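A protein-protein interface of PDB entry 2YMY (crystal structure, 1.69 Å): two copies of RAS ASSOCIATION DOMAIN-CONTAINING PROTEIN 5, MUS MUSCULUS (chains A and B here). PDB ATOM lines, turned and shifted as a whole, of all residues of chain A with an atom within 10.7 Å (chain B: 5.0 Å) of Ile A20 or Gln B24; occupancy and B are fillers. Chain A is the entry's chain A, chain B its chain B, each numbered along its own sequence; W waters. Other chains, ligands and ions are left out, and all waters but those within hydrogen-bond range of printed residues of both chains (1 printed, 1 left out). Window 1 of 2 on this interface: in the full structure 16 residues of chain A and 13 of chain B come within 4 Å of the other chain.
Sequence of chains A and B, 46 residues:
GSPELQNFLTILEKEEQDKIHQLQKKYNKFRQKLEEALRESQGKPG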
ATOM      1  N   LEU A  12     -14.033  -8.798  11.082  1.00  0.00           N
ATOM      2  CA  LEU A  12     -13.023  -7.766  11.227  1.00  0.00           C
ATOM      3  C   LEU A  12     -11.815  -8.100  10.371  1.00  0.00           C
ATOM      4  O   LEU A  12     -11.210  -7.213   9.763  1.00  0.00           O
ATOM      5  CB  LEU A  12     -12.571  -7.669  12.686  1.00  0.00           C
ATOM      6  CG  LEU A  12     -12.981  -6.512  13.595  1.00  0.00           C
ATOM      7  CD1 LEU A  12     -11.854  -6.251  14.625  1.00  0.00           C
ATOM      8  CD2 LEU A  12     -13.283  -5.262  12.811  1.00  0.00           C
ATOM      9  N   GLU A  13     -11.418  -9.370  10.354  1.00  0.00           N
ATOM     10  CA  GLU A  13     -10.239  -9.774   9.582  1.00  0.00           C
ATOM     11  C   GLU A  13     -10.504  -9.504   8.099  1.00  0.00           C
ATOM     12  O   GLU A  13      -9.614  -8.994   7.394  1.00  0.00           O
ATOM     13  CB  GLU A  13      -9.917 -11.257   9.820  1.00  0.00           C
ATOM     14  CG  GLU A  13      -9.336 -11.523  11.207  1.00  0.00           C
ATOM     15  CD  GLU A  13      -9.394 -12.977  11.647  1.00  0.00           C
ATOM     16  OE1 GLU A  13      -9.625 -13.871  10.796  1.00  0.00           O
ATOM     17  OE2 GLU A  13      -9.208 -13.218  12.869  1.00  0.00           O
ATOM     18  N   LYS A  14     -11.693  -9.813   7.623  1.00  0.00           N
ATOM     19  CA  LYS A  14     -12.001  -9.600   6.209  1.00  0.00           C
ATOM     20  C   LYS A  14     -11.984  -8.116   5.899  1.00  0.00           C
ATOM     21  O   LYS A  14     -11.431  -7.662   4.853  1.00  0.00           O
ATOM     22  CB  LYS A  14     -13.361 -10.196   5.829  1.00  0.00           C
ATOM     23  CG  LYS A  14     -13.730  -9.851   4.386  1.00  0.00           C
ATOM     24  CD  LYS A  14     -15.034 -10.506   3.979  1.00  0.00           C
ATOM     25  CE  LYS A  14     -15.587  -9.881   2.694  1.00  0.00           C
ATOM     26  NZ  LYS A  14     -14.586  -9.860   1.615  1.00  0.00           N
ATOM     27  N   GLU A  15     -12.585  -7.331   6.778  1.00  0.00           N
ATOM     28  CA  GLU A  15     -12.582  -5.878   6.568  1.00  0.00           C
ATOM     29  C   GLU A  15     -11.163  -5.302   6.453  1.00  0.00           C
ATOM     30  O   GLU A  15     -10.871  -4.512   5.535  1.00  0.00           O
ATOM     31  CB  GLU A  15     -13.393  -5.176   7.660  1.00  0.00           C
ATOM     32  CG  GLU A  15     -14.859  -5.404   7.411  1.00  0.00           C
ATOM     33  CD  GLU A  15     -15.750  -4.783   8.471  1.00  0.00           C
ATOM     34  OE1 GLU A  15     -15.360  -4.797   9.667  1.00  0.00           O
ATOM     35  OE2 GLU A  15     -16.845  -4.300   8.097  1.00  0.00           O
ATOM     36  N   GLU A  16     -10.297  -5.671   7.390  1.00  0.00           N
ATOM     37  CA  GLU A  16      -8.938  -5.124   7.430  1.00  0.00           C
ATOM     38  C   GLU A  16      -8.196  -5.602   6.187  1.00  0.00           C
ATOM     39  O   GLU A  16      -7.500  -4.826   5.511  1.00  0.00           O
ATOM     40  CB  GLU A  16      -8.198  -5.668   8.644  1.00  0.00           C
ATOM     41  CG  GLU A  16      -6.775  -5.159   8.743  1.00  0.00           C
ATOM     42  CD  GLU A  16      -6.011  -5.713   9.933  1.00  0.00           C
ATOM     43  OE1 GLU A  16      -6.525  -6.601  10.687  1.00  0.00           O
ATOM     44  OE2 GLU A  16      -4.884  -5.230  10.135  1.00  0.00           O
ATOM     45  N   GLN A  17      -8.278  -6.907   5.925  1.00  0.00           N
ATOM     46  CA  GLN A  17      -7.460  -7.458   4.841  1.00  0.00           C
ATOM     47  C   GLN A  17      -7.905  -6.903   3.486  1.00  0.00           C
ATOM     48  O   GLN A  17      -7.065  -6.581   2.611  1.00  0.00           O
ATOM     49  CB  GLN A  17      -7.483  -9.011   4.882  1.00  0.00           C
ATOM     50  CG  GLN A  17      -6.699  -9.529   6.048  1.00  0.00           C
ATOM     51  CD  GLN A  17      -6.952 -10.973   6.351  1.00  0.00           C
ATOM     52  OE1 GLN A  17      -7.261 -11.762   5.454  1.00  0.00           O
ATOM     53  NE2 GLN A  17      -6.851 -11.319   7.620  1.00  0.00           N
ATOM     54  N   ASP A  18      -9.213  -6.762   3.288  1.00  0.00           N
ATOM     55  CA  ASP A  18      -9.743  -6.199   2.041  1.00  0.00           C
ATOM     56  C   ASP A  18      -9.187  -4.781   1.834  1.00  0.00           C
ATOM     57  O   ASP A  18      -8.754  -4.416   0.716  1.00  0.00           O
ATOM     58  CB  ASP A  18     -11.282  -6.161   2.054  1.00  0.00           C
ATOM     59  CG  ASP A  18     -11.925  -7.539   1.809  1.00  0.00           C
ATOM     60  OD1 ASP A  18     -11.180  -8.516   1.562  1.00  0.00           O
ATOM     61  OD2 ASP A  18     -13.190  -7.650   1.873  1.00  0.00           O
ATOM     62  N   LYS A  19      -9.166  -3.982   2.895  1.00  0.00           N
ATOM     63  CA  LYS A  19      -8.673  -2.602   2.775  1.00  0.00           C
ATOM     64  C   LYS A  19      -7.184  -2.560   2.470  1.00  0.00           C
ATOM     65  O   LYS A  19      -6.719  -1.776   1.612  1.00  0.00           O
ATOM     66  CB  LYS A  19      -8.945  -1.815   4.030  1.00  0.00           C
ATOM     67  CG  LYS A  19     -10.381  -1.553   4.240  1.00  0.00           C
ATOM     68  CD  LYS A  19     -10.569  -0.803   5.508  1.00  0.00           C
ATOM     69  CE  LYS A  19     -12.036  -0.729   5.901  1.00  0.00           C
ATOM     70  NZ  LYS A  19     -12.127  -0.113   7.249  1.00  0.00           N
ATOM     71  N   ILE A  20      -6.413  -3.395   3.150  1.00  0.00           N
ATOM     72  CA  ILE A  20      -4.969  -3.441   2.894  1.00  0.00           C
ATOM     73  C   ILE A  20      -4.656  -3.942   1.474  1.00  0.00           C
ATOM     74  O   ILE A  20      -3.784  -3.387   0.772  1.00  0.00           O
ATOM     75  CB  ILE A  20      -4.231  -4.326   3.913  1.00  0.00           C
ATOM     76  CG1 ILE A  20      -4.323  -3.655   5.283  1.00  0.00           C
ATOM     77  CG2 ILE A  20      -2.738  -4.545   3.453  1.00  0.00           C
ATOM     78  CD1 ILE A  20      -3.795  -4.513   6.428  1.00  0.00           C
ATOM     79  N   HIS A  21      -5.380  -4.957   1.028  1.00  0.00           N
ATOM     80  CA  HIS A  21      -5.059  -5.577  -0.269  1.00  0.00           C
ATOM     81  C   HIS A  21      -5.476  -4.664  -1.396  1.00  0.00           C
ATOM     82  O   HIS A  21      -4.827  -4.653  -2.474  1.00  0.00           O
ATOM     83  CB  HIS A  21      -5.709  -6.936  -0.391  1.00  0.00           C
ATOM     84  CG  HIS A  21      -5.164  -7.918   0.583  1.00  0.00           C
ATOM     85  ND1 HIS A  21      -5.895  -8.990   1.045  1.00  0.00           N
ATOM     86  CD2 HIS A  21      -3.951  -8.004   1.169  1.00  0.00           C
ATOM     87  CE1 HIS A  21      -5.151  -9.689   1.880  1.00  0.00           C
ATOM     88  NE2 HIS A  21      -3.972  -9.113   1.979  1.00  0.00           N
ATOM     89  N   GLN A  22      -6.524  -3.877  -1.193  1.00  0.00           N
ATOM     90  CA  GLN A  22      -6.935  -2.932  -2.224  1.00  0.00           C
ATOM     91  C   GLN A  22      -5.915  -1.806  -2.331  1.00  0.00           C
ATOM     92  O   GLN A  22      -5.659  -1.300  -3.430  1.00  0.00           O
ATOM     93  CB  GLN A  22      -8.330  -2.364  -1.973  1.00  0.00           C
ATOM     94  CG  GLN A  22      -9.454  -3.376  -2.206  1.00  0.00           C
ATOM     95  CD  GLN A  22      -9.467  -3.936  -3.626  1.00  0.00           C
ATOM     96  OE1 GLN A  22      -9.459  -3.187  -4.612  1.00  0.00           O
ATOM     97  NE2 GLN A  22      -9.469  -5.260  -3.732  1.00  0.00           N
ATOM     98  N   LEU A  23      -5.337  -1.396  -1.206  1.00  0.00           N
ATOM     99  CA  LEU A  23      -4.263  -0.399  -1.264  1.00  0.00           C
ATOM    100  C   LEU A  23      -3.053  -0.948  -1.986  1.00  0.00           C
ATOM    101  O   LEU A  23      -2.441  -0.259  -2.855  1.00  0.00           O
ATOM    102  CB  LEU A  23      -3.895   0.034   0.170  1.00  0.00           C
ATOM    103  CG  LEU A  23      -3.374   1.442   0.470  1.00  0.00           C
ATOM    104  CD1 LEU A  23      -4.349   2.514   0.021  1.00  0.00           C
ATOM    105  CD2 LEU A  23      -3.108   1.587   1.970  1.00  0.00           C
ATOM    106  N   GLN A  24      -2.675  -2.181  -1.656  1.00  0.00           N
ATOM    107  CA  GLN A  24      -1.528  -2.811  -2.296  1.00  0.00           C
ATOM    108  C   GLN A  24      -1.773  -2.853  -3.806  1.00  0.00           C
ATOM    109  O   GLN A  24      -0.904  -2.489  -4.586  1.00  0.00           O
ATOM    110  CB  GLN A  24      -1.269  -4.219  -1.787  1.00  0.00           C
ATOM    111  CG  GLN A  24      -0.856  -4.298  -0.353  1.00  0.00           C
ATOM    112  CD  GLN A  24      -0.880  -5.722   0.143  1.00  0.00           C
ATOM    113  OE1 GLN A  24      -1.568  -6.570  -0.424  1.00  0.00           O
ATOM    114  NE2 GLN A  24      -0.106  -6.003   1.190  1.00  0.00           N
ATOM    115  N   LYS A  25      -2.964  -3.303  -4.211  1.00  0.00           N
ATOM    116  CA  LYS A  25      -3.327  -3.329  -5.635  1.00  0.00           C
ATOM    117  C   LYS A  25      -3.282  -1.947  -6.323  1.00  0.00           C
ATOM    118  O   LYS A  25      -2.751  -1.815  -7.445  1.00  0.00           O
ATOM    119  CB  LYS A  25      -4.717  -3.999  -5.806  1.00  0.00           C
ATOM    120  CG  LYS A  25      -4.984  -4.395  -7.262  1.00  0.00           C
ATOM    121  CD  LYS A  25      -6.194  -5.302  -7.427  1.00  0.00           C
ATOM    122  CE  LYS A  25      -6.494  -5.530  -8.917  1.00  0.00           C
ATOM    123  NZ  LYS A  25      -7.608  -6.504  -9.142  1.00  0.00           N
ATOM    124  N   LYS A  26      -3.782  -0.909  -5.667  1.00  0.00           N
ATOM    125  CA  LYS A  26      -3.841   0.422  -6.230  1.00  0.00           C
ATOM    126  C   LYS A  26      -2.436   0.945  -6.455  1.00  0.00           C
ATOM    127  O   LYS A  26      -2.112   1.479  -7.524  1.00  0.00           O
ATOM    128  CB  LYS A  26      -4.534   1.336  -5.246  1.00  0.00           C
ATOM    129  CG  LYS A  26      -4.879   2.718  -5.729  1.00  0.00           C
ATOM    130  CD  LYS A  26      -6.175   3.203  -5.045  1.00  0.00           C
ATOM    131  CE  LYS A  26      -6.015   4.547  -4.323  1.00  0.00           C
ATOM    132  NZ  LYS A  26      -5.655   5.687  -5.220  1.00  0.00           N
ATOM    133  N   TYR A  27      -1.587   0.778  -5.457  1.00  0.00           N
ATOM    134  CA  TYR A  27      -0.200   1.204  -5.675  1.00  0.00           C
ATOM    135  C   TYR A  27       0.521   0.380  -6.741  1.00  0.00           C
ATOM    136  O   TYR A  27       1.314   0.936  -7.540  1.00  0.00           O
ATOM    137  CB  TYR A  27       0.620   1.173  -4.386  1.00  0.00           C
ATOM    138  CG  TYR A  27       0.404   2.349  -3.488  1.00  0.00           C
ATOM    139  CD1 TYR A  27       1.135   3.520  -3.640  1.00  0.00           C
ATOM    140  CD2 TYR A  27      -0.495   2.285  -2.446  1.00  0.00           C
ATOM    141  CE1 TYR A  27       0.949   4.604  -2.783  1.00  0.00           C
ATOM    142  CE2 TYR A  27      -0.677   3.374  -1.586  1.00  0.00           C
ATOM    143  CZ  TYR A  27       0.020   4.515  -1.754  1.00  0.00           C
ATOM    144  OH  TYR A  27      -0.133   5.615  -0.915  1.00  0.00           O
ATOM    145  N   ASN A  28       0.287  -0.932  -6.800  1.00  0.00           N
ATOM    146  CA  ASN A  28       1.005  -1.763  -7.746  1.00  0.00           C
ATOM    147  C   ASN A  28       0.528  -1.448  -9.167  1.00  0.00           C
ATOM    148  O   ASN A  28       1.341  -1.406 -10.082  1.00  0.00           O
ATOM    149  CB  ASN A  28       0.835  -3.264  -7.414  1.00  0.00           C
ATOM    150  CG  ASN A  28       1.867  -3.771  -6.395  1.00  0.00           C
ATOM    151  OD1 ASN A  28       2.940  -3.191  -6.243  1.00  0.00           O
ATOM    152  ND2 ASN A  28       1.550  -4.881  -5.720  1.00  0.00           N
ATOM    153  N   ARG A  31       2.203   1.806 -10.174  1.00  0.00           N
ATOM    154  CA  ARG A  31       3.616   1.644 -10.476  1.00  0.00           C
ATOM    155  C   ARG A  31       3.813   0.937 -11.807  1.00  0.00           C
ATOM    156  O   ARG A  31       4.723   1.284 -12.582  1.00  0.00           O
ATOM    157  CB  ARG A  31       4.317   0.825  -9.404  1.00  0.00           C
ATOM    158  CG  ARG A  31       4.494   1.519  -8.097  1.00  0.00           C
ATOM    159  CD  ARG A  31       4.944   0.460  -7.074  1.00  0.00           C
ATOM    160  NE  ARG A  31       5.011   1.059  -5.768  1.00  0.00           N
ATOM    161  CZ  ARG A  31       4.395   0.606  -4.692  1.00  0.00           C
ATOM    162  NH1 ARG A  31       3.654  -0.523  -4.730  1.00  0.00           N
ATOM    163  NH2 ARG A  31       4.550   1.290  -3.570  1.00  0.00           N
ATOM    164  N   ILE B  20      -0.654   1.504   5.398  1.00  0.00           N
ATOM    165  CA  ILE B  20      -0.907   0.142   5.766  1.00  0.00           C
ATOM    166  C   ILE B  20      -0.708  -0.009   7.285  1.00  0.00           C
ATOM    167  O   ILE B  20      -1.499  -0.667   7.967  1.00  0.00           O
ATOM    168  CB  ILE B  20      -0.009  -0.814   4.983  1.00  0.00           C
ATOM    169  CG1 ILE B  20      -0.523  -0.906   3.542  1.00  0.00           C
ATOM    170  CG2 ILE B  20      -0.002  -2.207   5.618  1.00  0.00           C
ATOM    171  CD1 ILE B  20       0.391  -1.696   2.576  1.00  0.00           C
ATOM    172  N   HIS B  21       0.354   0.588   7.815  1.00  0.00           N
ATOM    173  CA  HIS B  21       0.630   0.425   9.273  1.00  0.00           C
ATOM    174  C   HIS B  21      -0.448   1.100  10.099  1.00  0.00           C
ATOM    175  O   HIS B  21      -0.830   0.617  11.170  1.00  0.00           O
ATOM    176  CB  HIS B  21       1.978   1.036   9.646  1.00  0.00           C
ATOM    177  CG  HIS B  21       3.135   0.239   9.166  1.00  0.00           C
ATOM    178  ND1 HIS B  21       4.370   0.800   8.923  1.00  0.00           N
ATOM    179  CD2 HIS B  21       3.244  -1.073   8.850  1.00  0.00           C
ATOM    180  CE1 HIS B  21       5.194  -0.134   8.480  1.00  0.00           C
ATOM    181  NE2 HIS B  21       4.535  -1.279   8.423  1.00  0.00           N
ATOM    182  N   GLN B  22      -0.910   2.240   9.610  1.00  0.00           N
ATOM    183  CA  GLN B  22      -1.980   2.980  10.277  1.00  0.00           C
ATOM    184  C   GLN B  22      -3.240   2.115  10.346  1.00  0.00           C
ATOM    185  O   GLN B  22      -3.891   2.052  11.403  1.00  0.00           O
ATOM    186  CB  GLN B  22      -2.234   4.281   9.523  1.00  0.00           C
ATOM    187  CG  GLN B  22      -3.178   5.285  10.151  1.00  0.00           C
ATOM    188  CD  GLN B  22      -3.422   6.463   9.209  1.00  0.00           C
ATOM    189  OE1 GLN B  22      -3.257   6.341   7.987  1.00  0.00           O
ATOM    190  NE2 GLN B  22      -3.801   7.606   9.769  1.00  0.00           N
ATOM    191  N   LEU B  23      -3.569   1.424   9.250  1.00  0.00           N
ATOM    192  CA  LEU B  23      -4.718   0.511   9.232  1.00  0.00           C
ATOM    193  C   LEU B  23      -4.533  -0.657  10.210  1.00  0.00           C
ATOM    194  O   LEU B  23      -5.433  -1.054  10.946  1.00  0.00           O
ATOM    195  CB  LEU B  23      -4.925  -0.073   7.814  1.00  0.00           C
ATOM    196  CG  LEU B  23      -5.728   0.744   6.807  1.00  0.00           C
ATOM    197  CD1 LEU B  23      -5.537   0.164   5.396  1.00  0.00           C
ATOM    198  CD2 LEU B  23      -7.212   0.725   7.194  1.00  0.00           C
ATOM    199  N   GLN B  24      -3.342  -1.218  10.204  1.00  0.00           N
ATOM    200  CA  GLN B  24      -3.050  -2.363  11.041  1.00  0.00           C
ATOM    201  C   GLN B  24      -3.162  -1.959  12.515  1.00  0.00           C
ATOM    202  O   GLN B  24      -3.699  -2.731  13.338  1.00  0.00           O
ATOM    203  CB  GLN B  24      -1.654  -2.890  10.720  1.00  0.00           C
ATOM    204  CG  GLN B  24      -1.658  -3.715   9.436  1.00  0.00           C
ATOM    205  CD  GLN B  24      -0.304  -4.200   9.025  1.00  0.00           C
ATOM    206  OE1 GLN B  24       0.717  -3.610   9.395  1.00  0.00           O
ATOM    207  NE2 GLN B  24      -0.277  -5.280   8.244  1.00  0.00           N
ATOM    208  N   LYS B  25      -2.668  -0.767  12.826  1.00  0.00           N
ATOM    209  CA  LYS B  25      -2.724  -0.236  14.199  1.00  0.00           C
ATOM    210  C   LYS B  25      -4.181  -0.118  14.645  1.00  0.00           C
ATOM    211  O   LYS B  25      -4.551  -0.569  15.749  1.00  0.00           O
ATOM    212  CB  LYS B  25      -2.037   1.130  14.306  1.00  0.00           C
ATOM    213  CG  LYS B  25      -2.134   1.741  15.707  1.00  0.00           C
ATOM    214  CD  LYS B  25      -1.359   3.047  15.845  1.00  0.00           C
ATOM    215  CE  LYS B  25      -1.638   3.722  17.195  1.00  0.00           C
ATOM    216  NZ  LYS B  25      -0.939   5.029  17.331  1.00  0.00           N
ATOM    217  N   LYS B  26      -5.009   0.484  13.796  1.00  0.00           N
ATOM    218  CA  LYS B  26      -6.439   0.667  14.119  1.00  0.00           C
ATOM    219  C   LYS B  26      -7.167  -0.634  14.333  1.00  0.00           C
ATOM    220  O   LYS B  26      -7.937  -0.785  15.284  1.00  0.00           O
ATOM    221  CB  LYS B  26      -7.162   1.444  13.014  1.00  0.00           C
ATOM    222  CG  LYS B  26      -6.851   2.921  12.964  1.00  0.00           C
ATOM    223  CD  LYS B  26      -7.868   3.637  12.088  1.00  0.00           C
ATOM    224  CE  LYS B  26      -7.363   4.987  11.608  1.00  0.00           C
ATOM    225  NZ  LYS B  26      -7.809   5.244  10.208  1.00  0.00           N
ATOM    226  N   TYR B  27      -6.977  -1.577  13.424  1.00  0.00           N
ATOM    227  CA  TYR B  27      -7.659  -2.850  13.501  1.00  0.00           C
ATOM    228  C   TYR B  27      -7.132  -3.700  14.635  1.00  0.00           C
ATOM    229  O   TYR B  27      -7.878  -4.455  15.257  1.00  0.00           O
ATOM    230  CB  TYR B  27      -7.553  -3.574  12.158  1.00  0.00           C
ATOM    231  CG  TYR B  27      -8.683  -3.181  11.244  1.00  0.00           C
ATOM    232  CD1 TYR B  27      -9.946  -3.706  11.438  1.00  0.00           C
ATOM    233  CD2 TYR B  27      -8.505  -2.260  10.246  1.00  0.00           C
ATOM    234  CE1 TYR B  27     -10.994  -3.349  10.650  1.00  0.00           C
ATOM    235  CE2 TYR B  27      -9.571  -1.898   9.424  1.00  0.00           C
ATOM    236  CZ  TYR B  27     -10.803  -2.445   9.646  1.00  0.00           C
ATOM    237  OH  TYR B  27     -11.889  -2.125   8.864  1.00  0.00           O
ATOM    238  N   ASN B  28      -5.836  -3.547  14.970  1.00  0.00           N
ATOM    239  CA  ASN B  28      -5.342  -4.247  16.159  1.00  0.00           C
ATOM    240  C   ASN B  28      -6.012  -3.760  17.440  1.00  0.00           C
ATOM    241  O   ASN B  28      -6.379  -4.567  18.282  1.00  0.00           O
ATOM    242  CB  ASN B  28      -3.830  -4.129  16.286  1.00  0.00           C
ATOM    243  CG  ASN B  28      -3.102  -4.853  15.168  1.00  0.00           C
ATOM    244  OD1 ASN B  28      -3.657  -5.732  14.503  1.00  0.00           O
ATOM    245  ND2 ASN B  28      -1.845  -4.470  14.945  1.00  0.00           N
ATOM    246  N   LYS B  29      -6.176  -2.449  17.576  1.00  0.00           N
ATOM    247  CA  LYS B  29      -6.901  -1.925  18.719  1.00  0.00           C
ATOM    248  C   LYS B  29      -8.374  -2.387  18.684  1.00  0.00           C
ATOM    249  O   LYS B  29      -8.975  -2.758  19.714  1.00  0.00           O
ATOM    250  CB  LYS B  29      -6.841  -0.416  18.712  1.00  0.00           C
ATOM    251  CG  LYS B  29      -7.603   0.206  19.856  1.00  0.00           C
ATOM    252  CD  LYS B  29      -7.143  -0.391  21.192  1.00  0.00           C
ATOM    253  CE  LYS B  29      -5.652  -0.202  21.438  1.00  0.00           C
ATOM    254  NZ  LYS B  29      -5.314  -0.453  22.869  1.00  0.00           N
HETATM  255  O   HOH W   1     -14.379  -2.502   9.791  1.00  0.00           O
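Ile A20 touches Gln B24, but with the chains exchanged Gln A24 does not touch Ile B20 (4.1 Å). Leu A23 touches Ile B20, but with the chains exchanged Ile A20 does not touch Leu B23 (4.01 Å). Of the 7 pairs that touch across the chains among the printed residues, none has its exchanged pair printed and touching as well.
Of the printed residues of chain B, Ile A20 touches Gln B24. Gln B24 touches just these residues of chain A: Glu A16 and Ile A20. Of chain A, only Leu A23 comes within 4 Å of Ile B20. No residue of chain A comes within 4 Å of His B21. Asn B28 touches none of the printed residues of chain A. Printed residues of chain B within 4 Å of Leu A23: Ile B20. Printed residues of chain B within 4 Å of Lys A19: Tyr B27 (2.6 Å). The nearest printed residue of chain B that does not touch Glu A16 is Leu B23 (4.3 Å).
The side-chain hydroxyl (OH) of Tyr B27 is in hydrogen-bond range of the side-chain amino group (NZ) of Lys A19.
CE1 of Tyr B27 touches CD2 of Leu A12, 3.7 Å away. Glu A15 touches Tyr B27. CA of Gln B24 touches OE2 of Glu A16, at 3.5 Å. Tyr B27 touches Glu A16 (CB to CD, 3.5 Å). CG of Gln B24 touches CD1 of Ile A20, 3.8 Å away. Leu A23 touches Ile B20 (CD2 to CG1, 3.9 Å).
Water W1 lies within hydrogen-bond range of OE1 of Glu A15 (2.5 Å) and OH of Tyr B27 (2.7 Å).
Hydrophobic or aromatic side chains of chain A that line the printed part of chain B: Leu A12, Ile A20 and Leu A23. Hydrophobic or aromatic side chains of chain B that line the printed part of chain A: Ile B20 and Tyr B27. Among the printed residues, 7 pairs touch across the chains.
O of Gln B24 lies close to ND2 of Asn B28, at 3.0 Å.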
